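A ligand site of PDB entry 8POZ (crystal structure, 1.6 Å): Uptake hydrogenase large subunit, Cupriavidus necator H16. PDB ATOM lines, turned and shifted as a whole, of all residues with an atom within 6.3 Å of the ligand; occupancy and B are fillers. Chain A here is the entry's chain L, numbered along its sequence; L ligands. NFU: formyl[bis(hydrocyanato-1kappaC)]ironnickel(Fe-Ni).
The side-chain sulfur (SG) of Cys 600 is bound to an iron atom (FE) of the ligand (2.4 Å).
N of Thr 553 is in hydrogen-bond range of N2 of the ligand (3.0 Å).
The guanidinium group (NH1) of Arg 530 sits at hydrogen-bond distance from a nitrogen (N1) of the ligand.
NE2 of His 82 sits at hydrogen-bond distance from O3 of the ligand (3.5 Å).
The backbone NH (N) of Arg 530 lies within hydrogen-bond range of a nitrogen (N1) of the ligand (2.9 Å).
An oxygen (O3) of the ligand is in hydrogen-bond range of the side-chain sulfur (SG) of Cys 81 (3.3 Å).
NI of the ligand is bound by SG of Cys 78 (2.2 Å).
The side-chain sulfur (SG) of Cys 75 is bound to a nickel atom (NI) of the ligand, at 2.3 Å.
SG of Cys 597 is bound to NI of the ligand (2.2 Å).
A nitrogen (N2) of the ligand sits at hydrogen-bond distance from the side-chain hydroxyl of Thr 553 (2.8 Å).
N of Val 551 sits at hydrogen-bond distance from OG1 of Thr 554, at 3.2 Å.
The backbone NH (N) of Cys 597 is in hydrogen-bond range of the side-chain hydroxyl (OG1) of Thr 553, 3.1 Å away.
The side-chain carboxylate (OE1) of Glu 27 lies close to the side-chain sulfur (SG) of Cys 597 (3.5 Å).
O of Cys 78 is in hydrogen-bond range of SG of Cys 81.
The side-chain carboxylate of Asp 595 is in salt-bridge range of the guanidinium group of Arg 530, 2.9 Å away.
The side-chain carboxylate of Asp 117 lies within salt-bridge range of the guanidinium group of Arg 530.
SG of Cys 75 lies close to N of Val 77.
The side-chain sulfur of Cys 600 lies close to a ring nitrogen (NE2) of His 82 (3.2 Å).
The backbone nitrogen (N) of Pro 529 lies close to a nitrogen (N1) of the ligand, at 3.3 Å.
Merely in contact with the ligand: Ala 528, Leu 533, Val 551 and Pro 552.
Within 4 Å of the ligand: Cys 75, Cys 78, Cys 81, His 82, Ala 528, Pro 529, Arg 530, Leu 533, Val 551, Pro 552, Thr 553, Cys 597 and Cys 600.
The nearest printed residue that does not touch the ligand is Val 77 (4.7 Å).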
ATOM      1  N   GLU A  27     -37.155  -9.857  25.846  1.00  0.00           N
ATOM      2  CA  GLU A  27     -36.479  -9.756  27.143  1.00  0.00           C
ATOM      3  C   GLU A  27     -36.786  -8.377  27.690  1.00  0.00           C
ATOM      4  O   GLU A  27     -36.679  -7.379  26.969  1.00  0.00           O
ATOM      5  CB  GLU A  27     -34.974  -9.986  27.014  1.00  0.00           C
ATOM      6  CG  GLU A  27     -34.221 -10.056  28.336  1.00  0.00           C
ATOM      7  CD  GLU A  27     -34.243  -8.740  29.115  1.00  0.00           C
ATOM      8  OE1 GLU A  27     -34.150  -7.667  28.463  1.00  0.00           O
ATOM      9  OE2 GLU A  27     -34.354  -8.765  30.363  1.00  0.00           O
ATOM     10  N   ILE A  74     -26.302  -7.118  33.027  1.00  0.00           N
ATOM     11  CA  ILE A  74     -27.179  -6.337  32.173  1.00  0.00           C
ATOM     12  C   ILE A  74     -28.210  -7.265  31.532  1.00  0.00           C
ATOM     13  O   ILE A  74     -29.364  -6.887  31.371  1.00  0.00           O
ATOM     14  CB  ILE A  74     -26.399  -5.557  31.087  1.00  0.00           C
ATOM     15  CG1 ILE A  74     -25.627  -4.396  31.726  1.00  0.00           C
ATOM     16  CG2 ILE A  74     -27.330  -5.030  30.002  1.00  0.00           C
ATOM     17  CD1 ILE A  74     -24.618  -3.747  30.810  1.00  0.00           C
ATOM     18  N   CYS A  75     -27.811  -8.486  31.199  1.00  0.00           N
ATOM     19  CA  CYS A  75     -28.703  -9.395  30.476  1.00  0.00           C
ATOM     20  C   CYS A  75     -28.313 -10.863  30.594  1.00  0.00           C
ATOM     21  O   CYS A  75     -27.170 -11.238  30.321  1.00  0.00           O
ATOM     22  CB  CYS A  75     -28.737  -8.999  29.009  1.00  0.00           C
ATOM     23  SG  CYS A  75     -29.951  -9.932  28.058  1.00  0.00           S
ATOM     24  N   GLY A  76     -29.286 -11.684  30.995  1.00  0.00           N
ATOM     25  CA  GLY A  76     -29.110 -13.123  31.119  1.00  0.00           C
ATOM     26  C   GLY A  76     -29.460 -13.896  29.856  1.00  0.00           C
ATOM     27  O   GLY A  76     -29.237 -15.110  29.808  1.00  0.00           O
ATOM     28  N   VAL A  77     -29.996 -13.210  28.858  1.00  0.00           N
ATOM     29  CA  VAL A  77     -30.268 -13.790  27.551  1.00  0.00           C
ATOM     30  C   VAL A  77     -29.022 -13.709  26.685  1.00  0.00           C
ATOM     31  O   VAL A  77     -28.529 -14.735  26.217  1.00  0.00           O
ATOM     32  CB  VAL A  77     -31.453 -13.104  26.845  1.00  0.00           C
ATOM     33  CG1 VAL A  77     -31.741 -13.786  25.518  1.00  0.00           C
ATOM     34  CG2 VAL A  77     -32.691 -13.158  27.728  1.00  0.00           C
ATOM     35  N   CYS A  78     -28.494 -12.505  26.474  1.00  0.00           N
ATOM     36  CA  CYS A  78     -27.221 -12.344  25.757  1.00  0.00           C
ATOM     37  C   CYS A  78     -26.082 -12.448  26.764  1.00  0.00           C
ATOM     38  O   CYS A  78     -25.205 -11.590  26.882  1.00  0.00           O
ATOM     39  CB  CYS A  78     -27.192 -11.048  24.934  1.00  0.00           C
ATOM     40  SG  CYS A  78     -27.453  -9.510  25.844  1.00  0.00           S
ATOM     41  N   THR A  79     -26.096 -13.570  27.479  1.00  0.00           N
ATOM     42  CA  THR A  79     -25.243 -13.757  28.656  1.00  0.00           C
ATOM     43  C   THR A  79     -23.796 -13.967  28.256  1.00  0.00           C
ATOM     44  O   THR A  79     -23.460 -14.898  27.508  1.00  0.00           O
ATOM     45  CB  THR A  79     -25.778 -14.905  29.561  1.00  0.00           C
ATOM     46  OG1 THR A  79     -24.961 -15.002  30.734  1.00  0.00           O
ATOM     47  CG2 THR A  79     -25.781 -16.250  28.857  1.00  0.00           C
ATOM     48  N   CYS A  81     -21.871 -11.616  26.560  1.00  0.00           N
ATOM     49  CA  CYS A  81     -21.423 -10.657  25.553  1.00  0.00           C
ATOM     50  C   CYS A  81     -20.959  -9.354  26.212  1.00  0.00           C
ATOM     51  O   CYS A  81     -19.990  -8.770  25.759  1.00  0.00           O
ATOM     52  CB  CYS A  81     -22.444 -10.423  24.442  1.00  0.00           C
ATOM     53  SG  CYS A  81     -23.902  -9.428  24.841  1.00  0.00           S
ATOM     54  N   HIS A  82     -21.640  -8.926  27.277  1.00  0.00           N
ATOM     55  CA  HIS A  82     -21.217  -7.738  28.042  1.00  0.00           C
ATOM     56  C   HIS A  82     -19.911  -7.985  28.799  1.00  0.00           C
ATOM     57  O   HIS A  82     -19.079  -7.088  28.909  1.00  0.00           O
ATOM     58  CB  HIS A  82     -22.308  -7.295  29.006  1.00  0.00           C
ATOM     59  CG  HIS A  82     -23.504  -6.725  28.311  1.00  0.00           C
ATOM     60  ND1 HIS A  82     -23.489  -5.482  27.730  1.00  0.00           N
ATOM     61  CD2 HIS A  82     -24.737  -7.230  28.094  1.00  0.00           C
ATOM     62  CE1 HIS A  82     -24.673  -5.241  27.189  1.00  0.00           C
ATOM     63  NE2 HIS A  82     -25.440  -6.292  27.390  1.00  0.00           N
ATOM     64  N   ASP A 117     -28.845 -18.140  21.538  1.00  0.00           N
ATOM     65  CA  ASP A 117     -29.691 -16.967  21.567  1.00  0.00           C
ATOM     66  C   ASP A 117     -30.587 -16.921  20.318  1.00  0.00           C
ATOM     67  O   ASP A 117     -31.811 -16.757  20.440  1.00  0.00           O
ATOM     68  CB  ASP A 117     -28.813 -15.721  21.697  1.00  0.00           C
ATOM     69  CG  ASP A 117     -29.513 -14.565  22.350  1.00  0.00           C
ATOM     70  OD1 ASP A 117     -30.753 -14.449  22.216  1.00  0.00           O
ATOM     71  OD2 ASP A 117     -28.812 -13.755  22.991  1.00  0.00           O
ATOM     72  N   ALA A 528     -22.688  -8.591  19.249  1.00  0.00           N
ATOM     73  CA  ALA A 528     -23.616  -9.306  20.116  1.00  0.00           C
ATOM     74  C   ALA A 528     -24.752  -9.883  19.255  1.00  0.00           C
ATOM     75  O   ALA A 528     -24.958  -9.436  18.118  1.00  0.00           O
ATOM     76  CB  ALA A 528     -24.177  -8.365  21.164  1.00  0.00           C
ATOM     77  N   PRO A 529     -25.491 -10.881  19.791  1.00  0.00           N
ATOM     78  CA  PRO A 529     -26.564 -11.467  18.986  1.00  0.00           C
ATOM     79  C   PRO A 529     -27.500 -10.450  18.327  1.00  0.00           C
ATOM     80  O   PRO A 529     -27.931 -10.680  17.205  1.00  0.00           O
ATOM     81  CB  PRO A 529     -27.313 -12.349  20.001  1.00  0.00           C
ATOM     82  CG  PRO A 529     -26.224 -12.803  20.905  1.00  0.00           C
ATOM     83  CD  PRO A 529     -25.308 -11.613  21.055  1.00  0.00           C
ATOM     84  N   ARG A 530     -27.785  -9.335  18.986  1.00  0.00           N
ATOM     85  CA  ARG A 530     -28.744  -8.368  18.461  1.00  0.00           C
ATOM     86  C   ARG A 530     -28.114  -7.194  17.689  1.00  0.00           C
ATOM     87  O   ARG A 530     -28.825  -6.325  17.199  1.00  0.00           O
ATOM     88  CB  ARG A 530     -29.643  -7.855  19.597  1.00  0.00           C
ATOM     89  CG  ARG A 530     -30.550  -8.961  20.132  1.00  0.00           C
ATOM     90  CD  ARG A 530     -30.992  -8.737  21.563  1.00  0.00           C
ATOM     91  NE  ARG A 530     -31.780  -9.886  22.010  1.00  0.00           N
ATOM     92  CZ  ARG A 530     -31.273 -11.035  22.445  1.00  0.00           C
ATOM     93  NH1 ARG A 530     -29.951 -11.225  22.547  1.00  0.00           N
ATOM     94  NH2 ARG A 530     -32.096 -12.013  22.791  1.00  0.00           N
ATOM     95  N   GLY A 531     -26.782  -7.166  17.563  1.00  0.00           N
ATOM     96  CA  GLY A 531     -26.120  -6.110  16.802  1.00  0.00           C
ATOM     97  C   GLY A 531     -24.862  -5.588  17.472  1.00  0.00           C
ATOM     98  O   GLY A 531     -24.165  -6.313  18.173  1.00  0.00           O
ATOM     99  N   ALA A 532     -24.612  -4.300  17.269  1.00  0.00           N
ATOM    100  CA  ALA A 532     -23.367  -3.653  17.653  1.00  0.00           C
ATOM    101  C   ALA A 532     -23.351  -3.280  19.132  1.00  0.00           C
ATOM    102  O   ALA A 532     -24.158  -2.469  19.591  1.00  0.00           O
ATOM    103  CB  ALA A 532     -23.161  -2.419  16.783  1.00  0.00           C
ATOM    104  N   LEU A 533     -22.422  -3.882  19.875  1.00  0.00           N
ATOM    105  CA  LEU A 533     -22.257  -3.606  21.313  1.00  0.00           C
ATOM    106  C   LEU A 533     -20.911  -2.942  21.544  1.00  0.00           C
ATOM    107  O   LEU A 533     -19.897  -3.383  21.015  1.00  0.00           O
ATOM    108  CB  LEU A 533     -22.305  -4.898  22.115  1.00  0.00           C
ATOM    109  CG  LEU A 533     -21.947  -4.805  23.608  1.00  0.00           C
ATOM    110  CD1 LEU A 533     -22.887  -3.878  24.357  1.00  0.00           C
ATOM    111  CD2 LEU A 533     -21.959  -6.199  24.228  1.00  0.00           C
ATOM    112  N   VAL A 551     -25.670  -0.387  23.490  1.00  0.00           N
ATOM    113  CA  VAL A 551     -26.018  -1.788  23.321  1.00  0.00           C
ATOM    114  C   VAL A 551     -26.890  -1.917  22.059  1.00  0.00           C
ATOM    115  O   VAL A 551     -27.471  -0.929  21.623  1.00  0.00           O
ATOM    116  CB  VAL A 551     -26.709  -2.245  24.633  1.00  0.00           C
ATOM    117  CG1 VAL A 551     -26.961  -3.735  24.666  1.00  0.00           C
ATOM    118  CG2 VAL A 551     -25.867  -1.855  25.847  1.00  0.00           C
ATOM    119  N   PRO A 552     -26.944  -3.108  21.426  1.00  0.00           N
ATOM    120  CA  PRO A 552     -27.672  -3.177  20.164  1.00  0.00           C
ATOM    121  C   PRO A 552     -29.111  -2.690  20.216  1.00  0.00           C
ATOM    122  O   PRO A 552     -29.540  -1.977  19.312  1.00  0.00           O
ATOM    123  CB  PRO A 552     -27.634  -4.668  19.822  1.00  0.00           C
ATOM    124  CG  PRO A 552     -26.410  -5.177  20.495  1.00  0.00           C
ATOM    125  CD  PRO A 552     -26.228  -4.356  21.727  1.00  0.00           C
ATOM    126  N   THR A 553     -29.847  -3.070  21.268  1.00  0.00           N
ATOM    127  CA  THR A 553     -31.264  -2.695  21.343  1.00  0.00           C
ATOM    128  C   THR A 553     -31.361  -1.206  21.719  1.00  0.00           C
ATOM    129  O   THR A 553     -32.403  -0.594  21.503  1.00  0.00           O
ATOM    130  CB  THR A 553     -32.090  -3.633  22.259  1.00  0.00           C
ATOM    131  OG1 THR A 553     -31.968  -4.979  21.779  1.00  0.00           O
ATOM    132  CG2 THR A 553     -33.571  -3.258  22.247  1.00  0.00           C
ATOM    133  N   THR A 554     -30.292  -0.609  22.240  1.00  0.00           N
ATOM    134  CA  THR A 554     -30.249   0.852  22.415  1.00  0.00           C
ATOM    135  C   THR A 554     -30.358   1.522  21.041  1.00  0.00           C
ATOM    136  O   THR A 554     -31.151   2.437  20.865  1.00  0.00           O
ATOM    137  CB  THR A 554     -28.987   1.376  23.131  1.00  0.00           C
ATOM    138  OG1 THR A 554     -28.666   0.531  24.247  1.00  0.00           O
ATOM    139  CG2 THR A 554     -29.199   2.811  23.626  1.00  0.00           C
ATOM    140  N   ASP A 595     -35.529  -9.068  17.774  1.00  0.00           N
ATOM    141  CA  ASP A 595     -35.156  -9.765  19.002  1.00  0.00           C
ATOM    142  C   ASP A 595     -34.860  -8.718  20.098  1.00  0.00           C
ATOM    143  O   ASP A 595     -33.743  -8.667  20.623  1.00  0.00           O
ATOM    144  CB  ASP A 595     -33.961 -10.683  18.682  1.00  0.00           C
ATOM    145  CG  ASP A 595     -33.485 -11.492  19.869  1.00  0.00           C
ATOM    146  OD1 ASP A 595     -34.188 -11.618  20.893  1.00  0.00           O
ATOM    147  OD2 ASP A 595     -32.360 -12.002  19.755  1.00  0.00           O
ATOM    148  N   PRO A 596     -35.862  -7.885  20.428  1.00  0.00           N
ATOM    149  CA  PRO A 596     -35.630  -6.812  21.385  1.00  0.00           C
ATOM    150  C   PRO A 596     -35.145  -7.302  22.744  1.00  0.00           C
ATOM    151  O   PRO A 596     -35.727  -8.216  23.322  1.00  0.00           O
ATOM    152  CB  PRO A 596     -37.015  -6.153  21.535  1.00  0.00           C
ATOM    153  CG  PRO A 596     -37.756  -6.539  20.308  1.00  0.00           C
ATOM    154  CD  PRO A 596     -37.265  -7.920  19.990  1.00  0.00           C
ATOM    155  N   CYS A 597     -34.064  -6.705  23.224  1.00  0.00           N
ATOM    156  CA  CYS A 597     -33.583  -6.987  24.558  1.00  0.00           C
ATOM    157  C   CYS A 597     -33.614  -5.668  25.327  1.00  0.00           C
ATOM    158  O   CYS A 597     -32.732  -4.826  25.186  1.00  0.00           O
ATOM    159  CB  CYS A 597     -32.192  -7.582  24.514  1.00  0.00           C
ATOM    160  SG  CYS A 597     -31.686  -8.278  26.095  1.00  0.00           S
ATOM    161  N   LEU A 598     -34.655  -5.515  26.130  1.00  0.00           N
ATOM    162  CA  LEU A 598     -34.937  -4.215  26.753  1.00  0.00           C
ATOM    163  C   LEU A 598     -34.082  -3.934  27.979  1.00  0.00           C
ATOM    164  O   LEU A 598     -33.727  -2.780  28.218  1.00  0.00           O
ATOM    165  CB  LEU A 598     -36.426  -4.052  27.073  1.00  0.00           C
ATOM    166  CG  LEU A 598     -37.274  -3.589  25.889  1.00  0.00           C
ATOM    167  CD1 LEU A 598     -37.020  -2.119  25.589  1.00  0.00           C
ATOM    168  CD2 LEU A 598     -37.053  -4.440  24.636  1.00  0.00           C
ATOM    169  N   ALA A 599     -33.747  -4.968  28.730  1.00  0.00           N
ATOM    170  CA  ALA A 599     -32.808  -4.809  29.843  1.00  0.00           C
ATOM    171  C   ALA A 599     -31.450  -4.368  29.307  1.00  0.00           C
ATOM    172  O   ALA A 599     -30.800  -3.490  29.864  1.00  0.00           O
ATOM    173  CB  ALA A 599     -32.678  -6.093  30.641  1.00  0.00           C
ATOM    174  N   CYS A 600     -31.025  -4.979  28.206  1.00  0.00           N
ATOM    175  CA  CYS A 600     -29.843  -4.546  27.481  1.00  0.00           C
ATOM    176  C   CYS A 600     -29.907  -3.100  27.036  1.00  0.00           C
ATOM    177  O   CYS A 600     -28.943  -2.344  27.196  1.00  0.00           O
ATOM    178  CB  CYS A 600     -29.652  -5.397  26.226  1.00  0.00           C
ATOM    179  SG  CYS A 600     -28.431  -6.694  26.458  1.00  0.00           S
ATOM    180  N   SER A 601     -31.042  -2.715  26.466  1.00  0.00           N
ATOM    181  CA  SER A 601     -31.174  -1.410  25.837  1.00  0.00           C
ATOM    182  C   SER A 601     -30.987  -0.259  26.824  1.00  0.00           C
ATOM    183  O   SER A 601     -30.486   0.795  26.457  1.00  0.00           O
ATOM    184  CB  SER A 601     -32.520  -1.270  25.120  1.00  0.00           C
ATOM    185  OG  SER A 601     -33.598  -1.079  26.023  1.00  0.00           O
HETATM  186 FE   NFU L   1     -27.954  -7.744  24.391  1.00  0.00          FE
HETATM  187 NI   NFU L   1     -29.589  -8.908  26.075  1.00  0.00          NI
HETATM  188  C1  NFU L   1     -27.654  -8.743  22.763  1.00  0.00           C
HETATM  189  N1  NFU L   1     -27.513  -9.291  21.854  1.00  0.00           N
HETATM  190  C2  NFU L   1     -28.926  -6.387  23.362  1.00  0.00           C
HETATM  191  N2  NFU L   1     -29.477  -5.609  22.774  1.00  0.00           N
HETATM  192  C3  NFU L   1     -26.321  -6.983  24.118  1.00  0.00           C
HETATM  193  O3  NFU L   1     -25.335  -6.537  23.945  1.00  0.00           O
